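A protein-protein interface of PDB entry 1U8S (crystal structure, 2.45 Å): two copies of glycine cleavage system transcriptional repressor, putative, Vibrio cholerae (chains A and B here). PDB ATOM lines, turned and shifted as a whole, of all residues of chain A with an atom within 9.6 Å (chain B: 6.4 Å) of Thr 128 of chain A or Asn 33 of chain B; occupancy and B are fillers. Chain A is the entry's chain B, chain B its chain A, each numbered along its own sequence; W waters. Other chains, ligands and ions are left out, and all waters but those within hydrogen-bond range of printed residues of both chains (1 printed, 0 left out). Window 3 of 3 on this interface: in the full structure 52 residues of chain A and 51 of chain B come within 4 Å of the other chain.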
ATOM      1  N   TYR A  97      21.876   4.432  39.762  1.00  0.00           N
ATOM      2  CA  TYR A  97      21.728   5.504  38.795  1.00  0.00           C
ATOM      3  C   TYR A  97      22.548   6.699  39.254  1.00  0.00           C
ATOM      4  O   TYR A  97      22.262   7.310  40.282  1.00  0.00           O
ATOM      5  CB  TYR A  97      20.265   5.912  38.645  1.00  0.00           C
ATOM      6  CG  TYR A  97      20.014   6.534  37.302  1.00  0.00           C
ATOM      7  CD1 TYR A  97      20.024   5.750  36.150  1.00  0.00           C
ATOM      8  CD2 TYR A  97      19.841   7.914  37.160  1.00  0.00           C
ATOM      9  CE1 TYR A  97      19.872   6.317  34.876  1.00  0.00           C
ATOM     10  CE2 TYR A  97      19.688   8.496  35.888  1.00  0.00           C
ATOM     11  CZ  TYR A  97      19.705   7.685  34.752  1.00  0.00           C
ATOM     12  OH  TYR A  97      19.551   8.221  33.497  1.00  0.00           O
ATOM     13  N   VAL A  98      23.573   7.026  38.483  1.00  0.00           N
ATOM     14  CA  VAL A  98      24.445   8.128  38.829  1.00  0.00           C
ATOM     15  C   VAL A  98      24.353   9.217  37.787  1.00  0.00           C
ATOM     16  O   VAL A  98      24.318   8.932  36.599  1.00  0.00           O
ATOM     17  CB  VAL A  98      25.913   7.640  38.937  1.00  0.00           C
ATOM     18  CG1 VAL A  98      26.857   8.823  39.154  1.00  0.00           C
ATOM     19  CG2 VAL A  98      26.038   6.638  40.079  1.00  0.00           C
ATOM     20  N   SER A 100      26.048  13.091  36.659  1.00  0.00           N
ATOM     21  CA  SER A 100      27.111  14.056  36.856  1.00  0.00           C
ATOM     22  C   SER A 100      27.165  15.023  35.693  1.00  0.00           C
ATOM     23  O   SER A 100      26.477  14.840  34.696  1.00  0.00           O
ATOM     24  CB  SER A 100      28.459  13.348  36.973  1.00  0.00           C
ATOM     25  OG  SER A 100      29.514  14.293  37.075  1.00  0.00           O
ATOM     26  N   ASP A 101      27.981  16.060  35.818  1.00  0.00           N
ATOM     27  CA  ASP A 101      28.123  17.018  34.736  1.00  0.00           C
ATOM     28  C   ASP A 101      29.449  16.724  34.051  1.00  0.00           C
ATOM     29  O   ASP A 101      29.663  17.110  32.910  1.00  0.00           O
ATOM     30  CB  ASP A 101      28.129  18.443  35.271  1.00  0.00           C
ATOM     31  CG  ASP A 101      29.301  18.706  36.189  1.00  0.00           C
ATOM     32  OD1 ASP A 101      29.346  18.101  37.283  1.00  0.00           O
ATOM     33  OD2 ASP A 101      30.172  19.513  35.807  1.00  0.00           O
ATOM     34  N   ASP A 102      30.333  16.039  34.772  1.00  0.00           N
ATOM     35  CA  ASP A 102      31.651  15.653  34.263  1.00  0.00           C
ATOM     36  C   ASP A 102      31.632  14.154  34.030  1.00  0.00           C
ATOM     37  O   ASP A 102      31.195  13.408  34.904  1.00  0.00           O
ATOM     38  CB  ASP A 102      32.753  15.961  35.291  1.00  0.00           C
ATOM     39  CG  ASP A 102      33.303  17.372  35.170  1.00  0.00           C
ATOM     40  OD1 ASP A 102      34.110  17.757  36.050  1.00  0.00           O
ATOM     41  OD2 ASP A 102      32.946  18.086  34.203  1.00  0.00           O
ATOM     42  N   LYS A 103      32.107  13.699  32.876  1.00  0.00           N
ATOM     43  CA  LYS A 103      32.107  12.264  32.636  1.00  0.00           C
ATOM     44  C   LYS A 103      33.497  11.659  32.806  1.00  0.00           C
ATOM     45  O   LYS A 103      33.648  10.441  32.841  1.00  0.00           O
ATOM     46  CB  LYS A 103      31.567  11.945  31.238  1.00  0.00           C
ATOM     47  CG  LYS A 103      32.550  12.148  30.094  1.00  0.00           C
ATOM     48  CD  LYS A 103      32.062  11.418  28.845  1.00  0.00           C
ATOM     49  CE  LYS A 103      33.091  11.431  27.720  1.00  0.00           C
ATOM     50  NZ  LYS A 103      32.648  10.599  26.560  1.00  0.00           N
ATOM     51  N   LEU A 104      34.503  12.517  32.933  1.00  0.00           N
ATOM     52  CA  LEU A 104      35.892  12.088  33.074  1.00  0.00           C
ATOM     53  C   LEU A 104      36.175  10.924  34.044  1.00  0.00           C
ATOM     54  O   LEU A 104      36.180  11.099  35.263  1.00  0.00           O
ATOM     55  CB  LEU A 104      36.751  13.295  33.465  1.00  0.00           C
ATOM     56  CG  LEU A 104      38.260  13.233  33.204  1.00  0.00           C
ATOM     57  CD1 LEU A 104      38.520  13.089  31.706  1.00  0.00           C
ATOM     58  CD2 LEU A 104      38.920  14.502  33.744  1.00  0.00           C
ATOM     59  N   THR A 107      32.610   6.478  35.124  1.00  0.00           N
ATOM     60  CA  THR A 107      31.995   5.164  35.015  1.00  0.00           C
ATOM     61  C   THR A 107      32.833   4.051  35.633  1.00  0.00           C
ATOM     62  O   THR A 107      32.311   3.235  36.387  1.00  0.00           O
ATOM     63  CB  THR A 107      31.676   4.787  33.546  1.00  0.00           C
ATOM     64  OG1 THR A 107      30.757   5.735  32.991  1.00  0.00           O
ATOM     65  CG2 THR A 107      31.035   3.401  33.485  1.00  0.00           C
ATOM     66  N   LEU A 124      25.033  -2.331  32.169  1.00  0.00           N
ATOM     67  CA  LEU A 124      25.557  -1.004  32.397  1.00  0.00           C
ATOM     68  C   LEU A 124      25.278  -0.108  31.207  1.00  0.00           C
ATOM     69  O   LEU A 124      25.092  -0.579  30.097  1.00  0.00           O
ATOM     70  CB  LEU A 124      27.067  -1.102  32.657  1.00  0.00           C
ATOM     71  CG  LEU A 124      27.895   0.145  32.973  1.00  0.00           C
ATOM     72  CD1 LEU A 124      29.182  -0.246  33.692  1.00  0.00           C
ATOM     73  CD2 LEU A 124      28.198   0.889  31.684  1.00  0.00           C
ATOM     74  N   SER A 125      25.214   1.187  31.468  1.00  0.00           N
ATOM     75  CA  SER A 125      25.005   2.204  30.450  1.00  0.00           C
ATOM     76  C   SER A 125      25.621   3.474  31.042  1.00  0.00           C
ATOM     77  O   SER A 125      25.418   3.784  32.220  1.00  0.00           O
ATOM     78  CB  SER A 125      23.514   2.419  30.153  1.00  0.00           C
ATOM     79  OG  SER A 125      22.851   3.170  31.164  1.00  0.00           O
ATOM     80  N   ALA A 126      26.411   4.171  30.231  1.00  0.00           N
ATOM     81  CA  ALA A 126      27.069   5.408  30.633  1.00  0.00           C
ATOM     82  C   ALA A 126      27.000   6.267  29.384  1.00  0.00           C
ATOM     83  O   ALA A 126      27.573   5.918  28.358  1.00  0.00           O
ATOM     84  CB  ALA A 126      28.510   5.131  31.018  1.00  0.00           C
ATOM     85  N   GLN A 127      26.300   7.390  29.464  1.00  0.00           N
ATOM     86  CA  GLN A 127      26.138   8.227  28.289  1.00  0.00           C
ATOM     87  C   GLN A 127      25.792   9.667  28.602  1.00  0.00           C
ATOM     88  O   GLN A 127      25.312   9.988  29.681  1.00  0.00           O
ATOM     89  CB  GLN A 127      25.027   7.634  27.407  1.00  0.00           C
ATOM     90  CG  GLN A 127      23.633   7.723  28.025  1.00  0.00           C
ATOM     91  CD  GLN A 127      22.649   6.717  27.444  1.00  0.00           C
ATOM     92  OE1 GLN A 127      22.441   6.663  26.232  1.00  0.00           O
ATOM     93  NE2 GLN A 127      22.031   5.913  28.317  1.00  0.00           N
ATOM     94  N   THR A 128      26.042  10.531  27.633  1.00  0.00           N
ATOM     95  CA  THR A 128      25.727  11.946  27.743  1.00  0.00           C
ATOM     96  C   THR A 128      24.309  12.059  27.176  1.00  0.00           C
ATOM     97  O   THR A 128      24.022  11.484  26.127  1.00  0.00           O
ATOM     98  CB  THR A 128      26.671  12.791  26.877  1.00  0.00           C
ATOM     99  OG1 THR A 128      28.020  12.640  27.339  1.00  0.00           O
ATOM    100  CG2 THR A 128      26.265  14.253  26.924  1.00  0.00           C
ATOM    101  N   ILE A 129      23.427  12.784  27.861  1.00  0.00           N
ATOM    102  CA  ILE A 129      22.051  12.936  27.396  1.00  0.00           C
ATOM    103  C   ILE A 129      21.846  14.251  26.636  1.00  0.00           C
ATOM    104  O   ILE A 129      22.572  15.222  26.864  1.00  0.00           O
ATOM    105  CB  ILE A 129      21.056  12.891  28.576  1.00  0.00           C
ATOM    106  CG1 ILE A 129      21.432  11.762  29.540  1.00  0.00           C
ATOM    107  CG2 ILE A 129      19.640  12.637  28.052  1.00  0.00           C
ATOM    108  CD1 ILE A 129      21.281  10.368  28.956  1.00  0.00           C
ATOM    109  N   SER A 130      20.848  14.256  25.746  1.00  0.00           N
ATOM    110  CA  SER A 130      20.455  15.394  24.885  1.00  0.00           C
ATOM    111  C   SER A 130      20.911  16.821  25.241  1.00  0.00           C
ATOM    112  O   SER A 130      21.997  17.256  24.847  1.00  0.00           O
ATOM    113  CB  SER A 130      18.926  15.395  24.716  1.00  0.00           C
ATOM    114  OG  SER A 130      18.494  16.421  23.834  1.00  0.00           O
ATOM    115  N   LYS A 131      20.056  17.552  25.958  1.00  0.00           N
ATOM    116  CA  LYS A 131      20.340  18.929  26.361  1.00  0.00           C
ATOM    117  C   LYS A 131      19.233  19.428  27.292  1.00  0.00           C
ATOM    118  O   LYS A 131      18.054  19.418  26.932  1.00  0.00           O
ATOM    119  CB  LYS A 131      20.407  19.839  25.128  1.00  0.00           C
ATOM    120  CG  LYS A 131      20.750  21.303  25.431  1.00  0.00           C
ATOM    121  CD  LYS A 131      22.254  21.525  25.542  1.00  0.00           C
ATOM    122  CE  LYS A 131      22.594  22.944  26.012  1.00  0.00           C
ATOM    123  NZ  LYS A 131      22.296  23.160  27.467  1.00  0.00           N
ATOM    124  N   ASN A 139      23.929  18.403  28.645  1.00  0.00           N
ATOM    125  CA  ASN A 139      25.316  18.477  29.095  1.00  0.00           C
ATOM    126  C   ASN A 139      25.580  17.628  30.342  1.00  0.00           C
ATOM    127  O   ASN A 139      26.588  17.818  31.030  1.00  0.00           O
ATOM    128  CB  ASN A 139      25.702  19.936  29.370  1.00  0.00           C
ATOM    129  CG  ASN A 139      24.724  20.629  30.296  1.00  0.00           C
ATOM    130  OD1 ASN A 139      23.546  20.794  29.963  1.00  0.00           O
ATOM    131  ND2 ASN A 139      25.204  21.035  31.469  1.00  0.00           N
ATOM    132  N   GLN A 140      24.675  16.698  30.635  1.00  0.00           N
ATOM    133  CA  GLN A 140      24.846  15.828  31.792  1.00  0.00           C
ATOM    134  C   GLN A 140      25.200  14.396  31.394  1.00  0.00           C
ATOM    135  O   GLN A 140      24.841  13.931  30.309  1.00  0.00           O
ATOM    136  CB  GLN A 140      23.583  15.819  32.649  1.00  0.00           C
ATOM    137  CG  GLN A 140      23.568  16.870  33.743  1.00  0.00           C
ATOM    138  CD  GLN A 140      22.317  16.784  34.585  1.00  0.00           C
ATOM    139  OE1 GLN A 140      22.003  15.735  35.142  1.00  0.00           O
ATOM    140  NE2 GLN A 140      21.589  17.889  34.680  1.00  0.00           N
ATOM    141  N   PHE A 141      25.904  13.703  32.281  1.00  0.00           N
ATOM    142  CA  PHE A 141      26.314  12.326  32.031  1.00  0.00           C
ATOM    143  C   PHE A 141      25.571  11.399  33.000  1.00  0.00           C
ATOM    144  O   PHE A 141      25.617  11.621  34.210  1.00  0.00           O
ATOM    145  CB  PHE A 141      27.824  12.205  32.243  1.00  0.00           C
ATOM    146  CG  PHE A 141      28.404  10.914  31.741  1.00  0.00           C
ATOM    147  CD1 PHE A 141      28.485  10.657  30.375  1.00  0.00           C
ATOM    148  CD2 PHE A 141      28.868   9.953  32.631  1.00  0.00           C
ATOM    149  CE1 PHE A 141      29.020   9.464  29.903  1.00  0.00           C
ATOM    150  CE2 PHE A 141      29.400   8.759  32.168  1.00  0.00           C
ATOM    151  CZ  PHE A 141      29.476   8.516  30.798  1.00  0.00           C
ATOM    152  N   HIS A 142      24.883  10.382  32.470  1.00  0.00           N
ATOM    153  CA  HIS A 142      24.136   9.433  33.306  1.00  0.00           C
ATOM    154  C   HIS A 142      24.669   7.999  33.222  1.00  0.00           C
ATOM    155  O   HIS A 142      24.862   7.452  32.132  1.00  0.00           O
ATOM    156  CB  HIS A 142      22.640   9.398  32.933  1.00  0.00           C
ATOM    157  CG  HIS A 142      21.918  10.696  33.135  1.00  0.00           C
ATOM    158  ND1 HIS A 142      20.542  10.777  33.210  1.00  0.00           N
ATOM    159  CD2 HIS A 142      22.372  11.969  33.249  1.00  0.00           C
ATOM    160  CE1 HIS A 142      20.182  12.039  33.361  1.00  0.00           C
ATOM    161  NE2 HIS A 142      21.273  12.784  33.388  1.00  0.00           N
ATOM    162  N   ILE A 143      24.892   7.391  34.379  1.00  0.00           N
ATOM    163  CA  ILE A 143      25.373   6.012  34.455  1.00  0.00           C
ATOM    164  C   ILE A 143      24.252   5.147  35.032  1.00  0.00           C
ATOM    165  O   ILE A 143      23.578   5.542  35.980  1.00  0.00           O
ATOM    166  CB  ILE A 143      26.639   5.904  35.370  1.00  0.00           C
ATOM    167  CG1 ILE A 143      27.787   6.726  34.765  1.00  0.00           C
ATOM    168  CG2 ILE A 143      27.066   4.443  35.535  1.00  0.00           C
ATOM    169  CD1 ILE A 143      29.071   6.754  35.609  1.00  0.00           C
ATOM    170  N   VAL B  27      36.190   2.642  25.561  1.00  0.00           N
ATOM    171  CA  VAL B  27      35.038   3.188  24.851  1.00  0.00           C
ATOM    172  C   VAL B  27      34.716   4.634  25.226  1.00  0.00           C
ATOM    173  O   VAL B  27      34.488   5.478  24.342  1.00  0.00           O
ATOM    174  CB  VAL B  27      33.786   2.335  25.088  1.00  0.00           C
ATOM    175  CG1 VAL B  27      32.617   2.940  24.374  1.00  0.00           C
ATOM    176  CG2 VAL B  27      34.021   0.923  24.603  1.00  0.00           C
ATOM    177  N   THR B  28      34.696   4.922  26.528  1.00  0.00           N
ATOM    178  CA  THR B  28      34.397   6.275  27.004  1.00  0.00           C
ATOM    179  C   THR B  28      35.485   7.296  26.647  1.00  0.00           C
ATOM    180  O   THR B  28      35.181   8.441  26.332  1.00  0.00           O
ATOM    181  CB  THR B  28      34.158   6.290  28.537  1.00  0.00           C
ATOM    182  OG1 THR B  28      35.278   5.694  29.194  1.00  0.00           O
ATOM    183  CG2 THR B  28      32.905   5.517  28.894  1.00  0.00           C
ATOM    184  N   GLY B  31      35.357   8.848  23.384  1.00  0.00           N
ATOM    185  CA  GLY B  31      34.252   9.782  23.243  1.00  0.00           C
ATOM    186  C   GLY B  31      32.915   9.150  22.910  1.00  0.00           C
ATOM    187  O   GLY B  31      31.992   9.841  22.474  1.00  0.00           O
ATOM    188  N   CYS B  32      32.793   7.843  23.116  1.00  0.00           N
ATOM    189  CA  CYS B  32      31.538   7.169  22.808  1.00  0.00           C
ATOM    190  C   CYS B  32      30.638   6.992  24.020  1.00  0.00           C
ATOM    191  O   CYS B  32      31.075   7.087  25.167  1.00  0.00           O
ATOM    192  CB  CYS B  32      31.805   5.809  22.168  1.00  0.00           C
ATOM    193  SG  CYS B  32      32.683   5.880  20.585  1.00  0.00           S
ATOM    194  N   ASN B  33      29.366   6.747  23.744  1.00  0.00           N
ATOM    195  CA  ASN B  33      28.373   6.532  24.775  1.00  0.00           C
ATOM    196  C   ASN B  33      28.054   5.049  24.830  1.00  0.00           C
ATOM    197  O   ASN B  33      28.064   4.367  23.803  1.00  0.00           O
ATOM    198  CB  ASN B  33      27.104   7.316  24.446  1.00  0.00           C
ATOM    199  CG  ASN B  33      27.245   8.802  24.729  1.00  0.00           C
ATOM    200  OD1 ASN B  33      26.532   9.622  24.149  1.00  0.00           O
ATOM    201  ND2 ASN B  33      28.154   9.156  25.636  1.00  0.00           N
ATOM    202  N   ILE B  34      27.797   4.546  26.030  1.00  0.00           N
ATOM    203  CA  ILE B  34      27.431   3.151  26.205  1.00  0.00           C
ATOM    204  C   ILE B  34      25.928   3.210  26.466  1.00  0.00           C
ATOM    205  O   ILE B  34      25.491   3.601  27.549  1.00  0.00           O
ATOM    206  CB  ILE B  34      28.169   2.524  27.414  1.00  0.00           C
ATOM    207  CG1 ILE B  34      29.674   2.539  27.158  1.00  0.00           C
ATOM    208  CG2 ILE B  34      27.719   1.096  27.633  1.00  0.00           C
ATOM    209  CD1 ILE B  34      30.513   2.067  28.341  1.00  0.00           C
ATOM    210  N   ILE B  35      25.140   2.836  25.459  1.00  0.00           N
ATOM    211  CA  ILE B  35      23.683   2.869  25.557  1.00  0.00           C
ATOM    212  C   ILE B  35      23.102   1.728  26.390  1.00  0.00           C
ATOM    213  O   ILE B  35      22.109   1.894  27.107  1.00  0.00           O
ATOM    214  CB  ILE B  35      23.056   2.845  24.151  1.00  0.00           C
ATOM    215  CG1 ILE B  35      23.571   4.037  23.341  1.00  0.00           C
ATOM    216  CG2 ILE B  35      21.536   2.912  24.238  1.00  0.00           C
ATOM    217  CD1 ILE B  35      23.251   3.921  21.855  1.00  0.00           C
ATOM    218  N   ASP B  36      23.731   0.568  26.310  1.00  0.00           N
ATOM    219  CA  ASP B  36      23.244  -0.581  27.055  1.00  0.00           C
ATOM    220  C   ASP B  36      24.312  -1.668  26.946  1.00  0.00           C
ATOM    221  O   ASP B  36      25.268  -1.535  26.178  1.00  0.00           O
ATOM    222  CB  ASP B  36      21.921  -1.054  26.448  1.00  0.00           C
ATOM    223  CG  ASP B  36      21.081  -1.859  27.418  1.00  0.00           C
ATOM    224  OD1 ASP B  36      21.440  -1.942  28.610  1.00  0.00           O
ATOM    225  OD2 ASP B  36      20.043  -2.401  26.985  1.00  0.00           O
ATOM    226  N   LEU B  51      26.265  -2.180  23.375  1.00  0.00           N
ATOM    227  CA  LEU B  51      25.838  -1.347  22.265  1.00  0.00           C
ATOM    228  C   LEU B  51      26.280   0.071  22.594  1.00  0.00           C
ATOM    229  O   LEU B  51      25.795   0.671  23.554  1.00  0.00           O
ATOM    230  CB  LEU B  51      24.315  -1.380  22.097  1.00  0.00           C
ATOM    231  CG  LEU B  51      23.819  -0.200  21.250  1.00  0.00           C
ATOM    232  CD1 LEU B  51      24.178  -0.440  19.772  1.00  0.00           C
ATOM    233  CD2 LEU B  51      22.328  -0.022  21.402  1.00  0.00           C
ATOM    234  N   ILE B  52      27.210   0.591  21.801  1.00  0.00           N
ATOM    235  CA  ILE B  52      27.734   1.937  21.998  1.00  0.00           C
ATOM    236  C   ILE B  52      27.370   2.747  20.765  1.00  0.00           C
ATOM    237  O   ILE B  52      26.909   2.190  19.771  1.00  0.00           O
ATOM    238  CB  ILE B  52      29.280   1.942  22.113  1.00  0.00           C
ATOM    239  CG1 ILE B  52      29.907   1.542  20.765  1.00  0.00           C
ATOM    240  CG2 ILE B  52      29.729   0.982  23.212  1.00  0.00           C
ATOM    241  CD1 ILE B  52      31.414   1.654  20.745  1.00  0.00           C
ATOM    242  N   SER B  53      27.591   4.054  20.834  1.00  0.00           N
ATOM    243  CA  SER B  53      27.297   4.948  19.726  1.00  0.00           C
ATOM    244  C   SER B  53      28.204   6.154  19.863  1.00  0.00           C
ATOM    245  O   SER B  53      28.691   6.458  20.955  1.00  0.00           O
ATOM    246  CB  SER B  53      25.850   5.410  19.774  1.00  0.00           C
ATOM    247  OG  SER B  53      25.637   6.248  20.897  1.00  0.00           O
ATOM    248  N   GLY B  54      28.425   6.846  18.755  1.00  0.00           N
ATOM    249  CA  GLY B  54      29.271   8.019  18.781  1.00  0.00           C
ATOM    250  C   GLY B  54      29.395   8.520  17.370  1.00  0.00           C
ATOM    251  O   GLY B  54      28.700   8.030  16.482  1.00  0.00           O
HETATM  252  O   HOH W   1      20.175   3.524  27.066  1.00  0.00           O
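NZ of Lys 103 of chain A sits at hydrogen-bond distance from O of Thr 28 of chain B (3.3 Å). ND2 of Asn 33 of chain B sits close to N of Thr 128 of chain A, at 3.2 Å. The backbone carbonyl oxygen of Ala 126 of chain A lies within hydrogen-bond range of the backbone NH of Ile 34 of chain B (2.7 Å).
The backbone NH (N) of Asn 33 of chain B lies within hydrogen-bond range of the backbone carbonyl oxygen (O) of Ser 53 of chain B (2.9 Å). N of Ile 35 of chain B sits at hydrogen-bond distance from O of Leu 51 of chain B, at 3.0 Å. O of Asp 36 of chain B is in hydrogen-bond range of N of Leu 51 of chain B, 3.0 Å away. The backbone carbonyl oxygen of Gln 127 of chain A sits at hydrogen-bond distance from the backbone NH of His 142 of chain A (2.8 Å).
Lys 103 of chain A touches Gly 31 of chain B (NZ to CA, 3.8 Å). Leu 124 of chain A touches Ile 34 of chain B (O to CG2, 3.97 Å). Leu 124 of chain A touches Asp 36 of chain B. Ser 125 of chain A touches Ile 34 of chain B. Ser 125 of chain A touches Ile 35 of chain B. Ala 126 of chain A touches Asn 33 of chain B (O to C, 3.7 Å). CA of Gln 127 of chain A touches ND2 of Asn 33 of chain B (3.5 Å).
Tyr 97 of chain A touches none of the printed residues of chain B. Of the printed residues of chain B, Leu 124 of chain A touches Ile 34 and Asp 36. Of the printed residues of chain B, Ser 125 of chain A touches Ile 34 (3.3 Å) and Ile 35 (3.4 Å). No residue of chain A comes within 4 Å of Cys 32 of chain B. Printed residues of chain A within 4 Å of Asp 36 of chain B: Leu 124 (3.4 Å). No residue of chain A comes within 4 Å of Ile 52 of chain B. No residue of chain A comes within 4 Å of Ser 53 of chain B. The nearest printed residue of chain B that does not touch Thr 128 of chain A is Ile 34 of chain B (6.4 Å). The nearest residue of chain A that does not touch Asn 33 of chain B is Phe 141 of chain A (4.4 Å).
Hydrophobic or aromatic side chains of chain B within 4 Å of the printed part of chain A: Ile 34. Of the 21 printed residues of chain A, 6 touch a printed residue of chain B. Printed residues of chain A that touch a printed residue of chain B: Lys 103, Leu 124, Ser 125, Ala 126, Gln 127 and Thr 128. Along chain A the printed residues that touch a printed residue of chain B span positions 103 to 128. Among the printed residues, no Asp or Glu carboxylate lies within 4 Å of a Lys or Arg side-chain nitrogen of the other chain.
No position is printed for both chains.
Water W1 lies within hydrogen-bond range of the backbone carbonyl oxygen (O) of Ile 35 of chain B (2.5 Å) and the side-chain amide nitrogen (NE2) of Gln 127 of chain A (3.3 Å).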
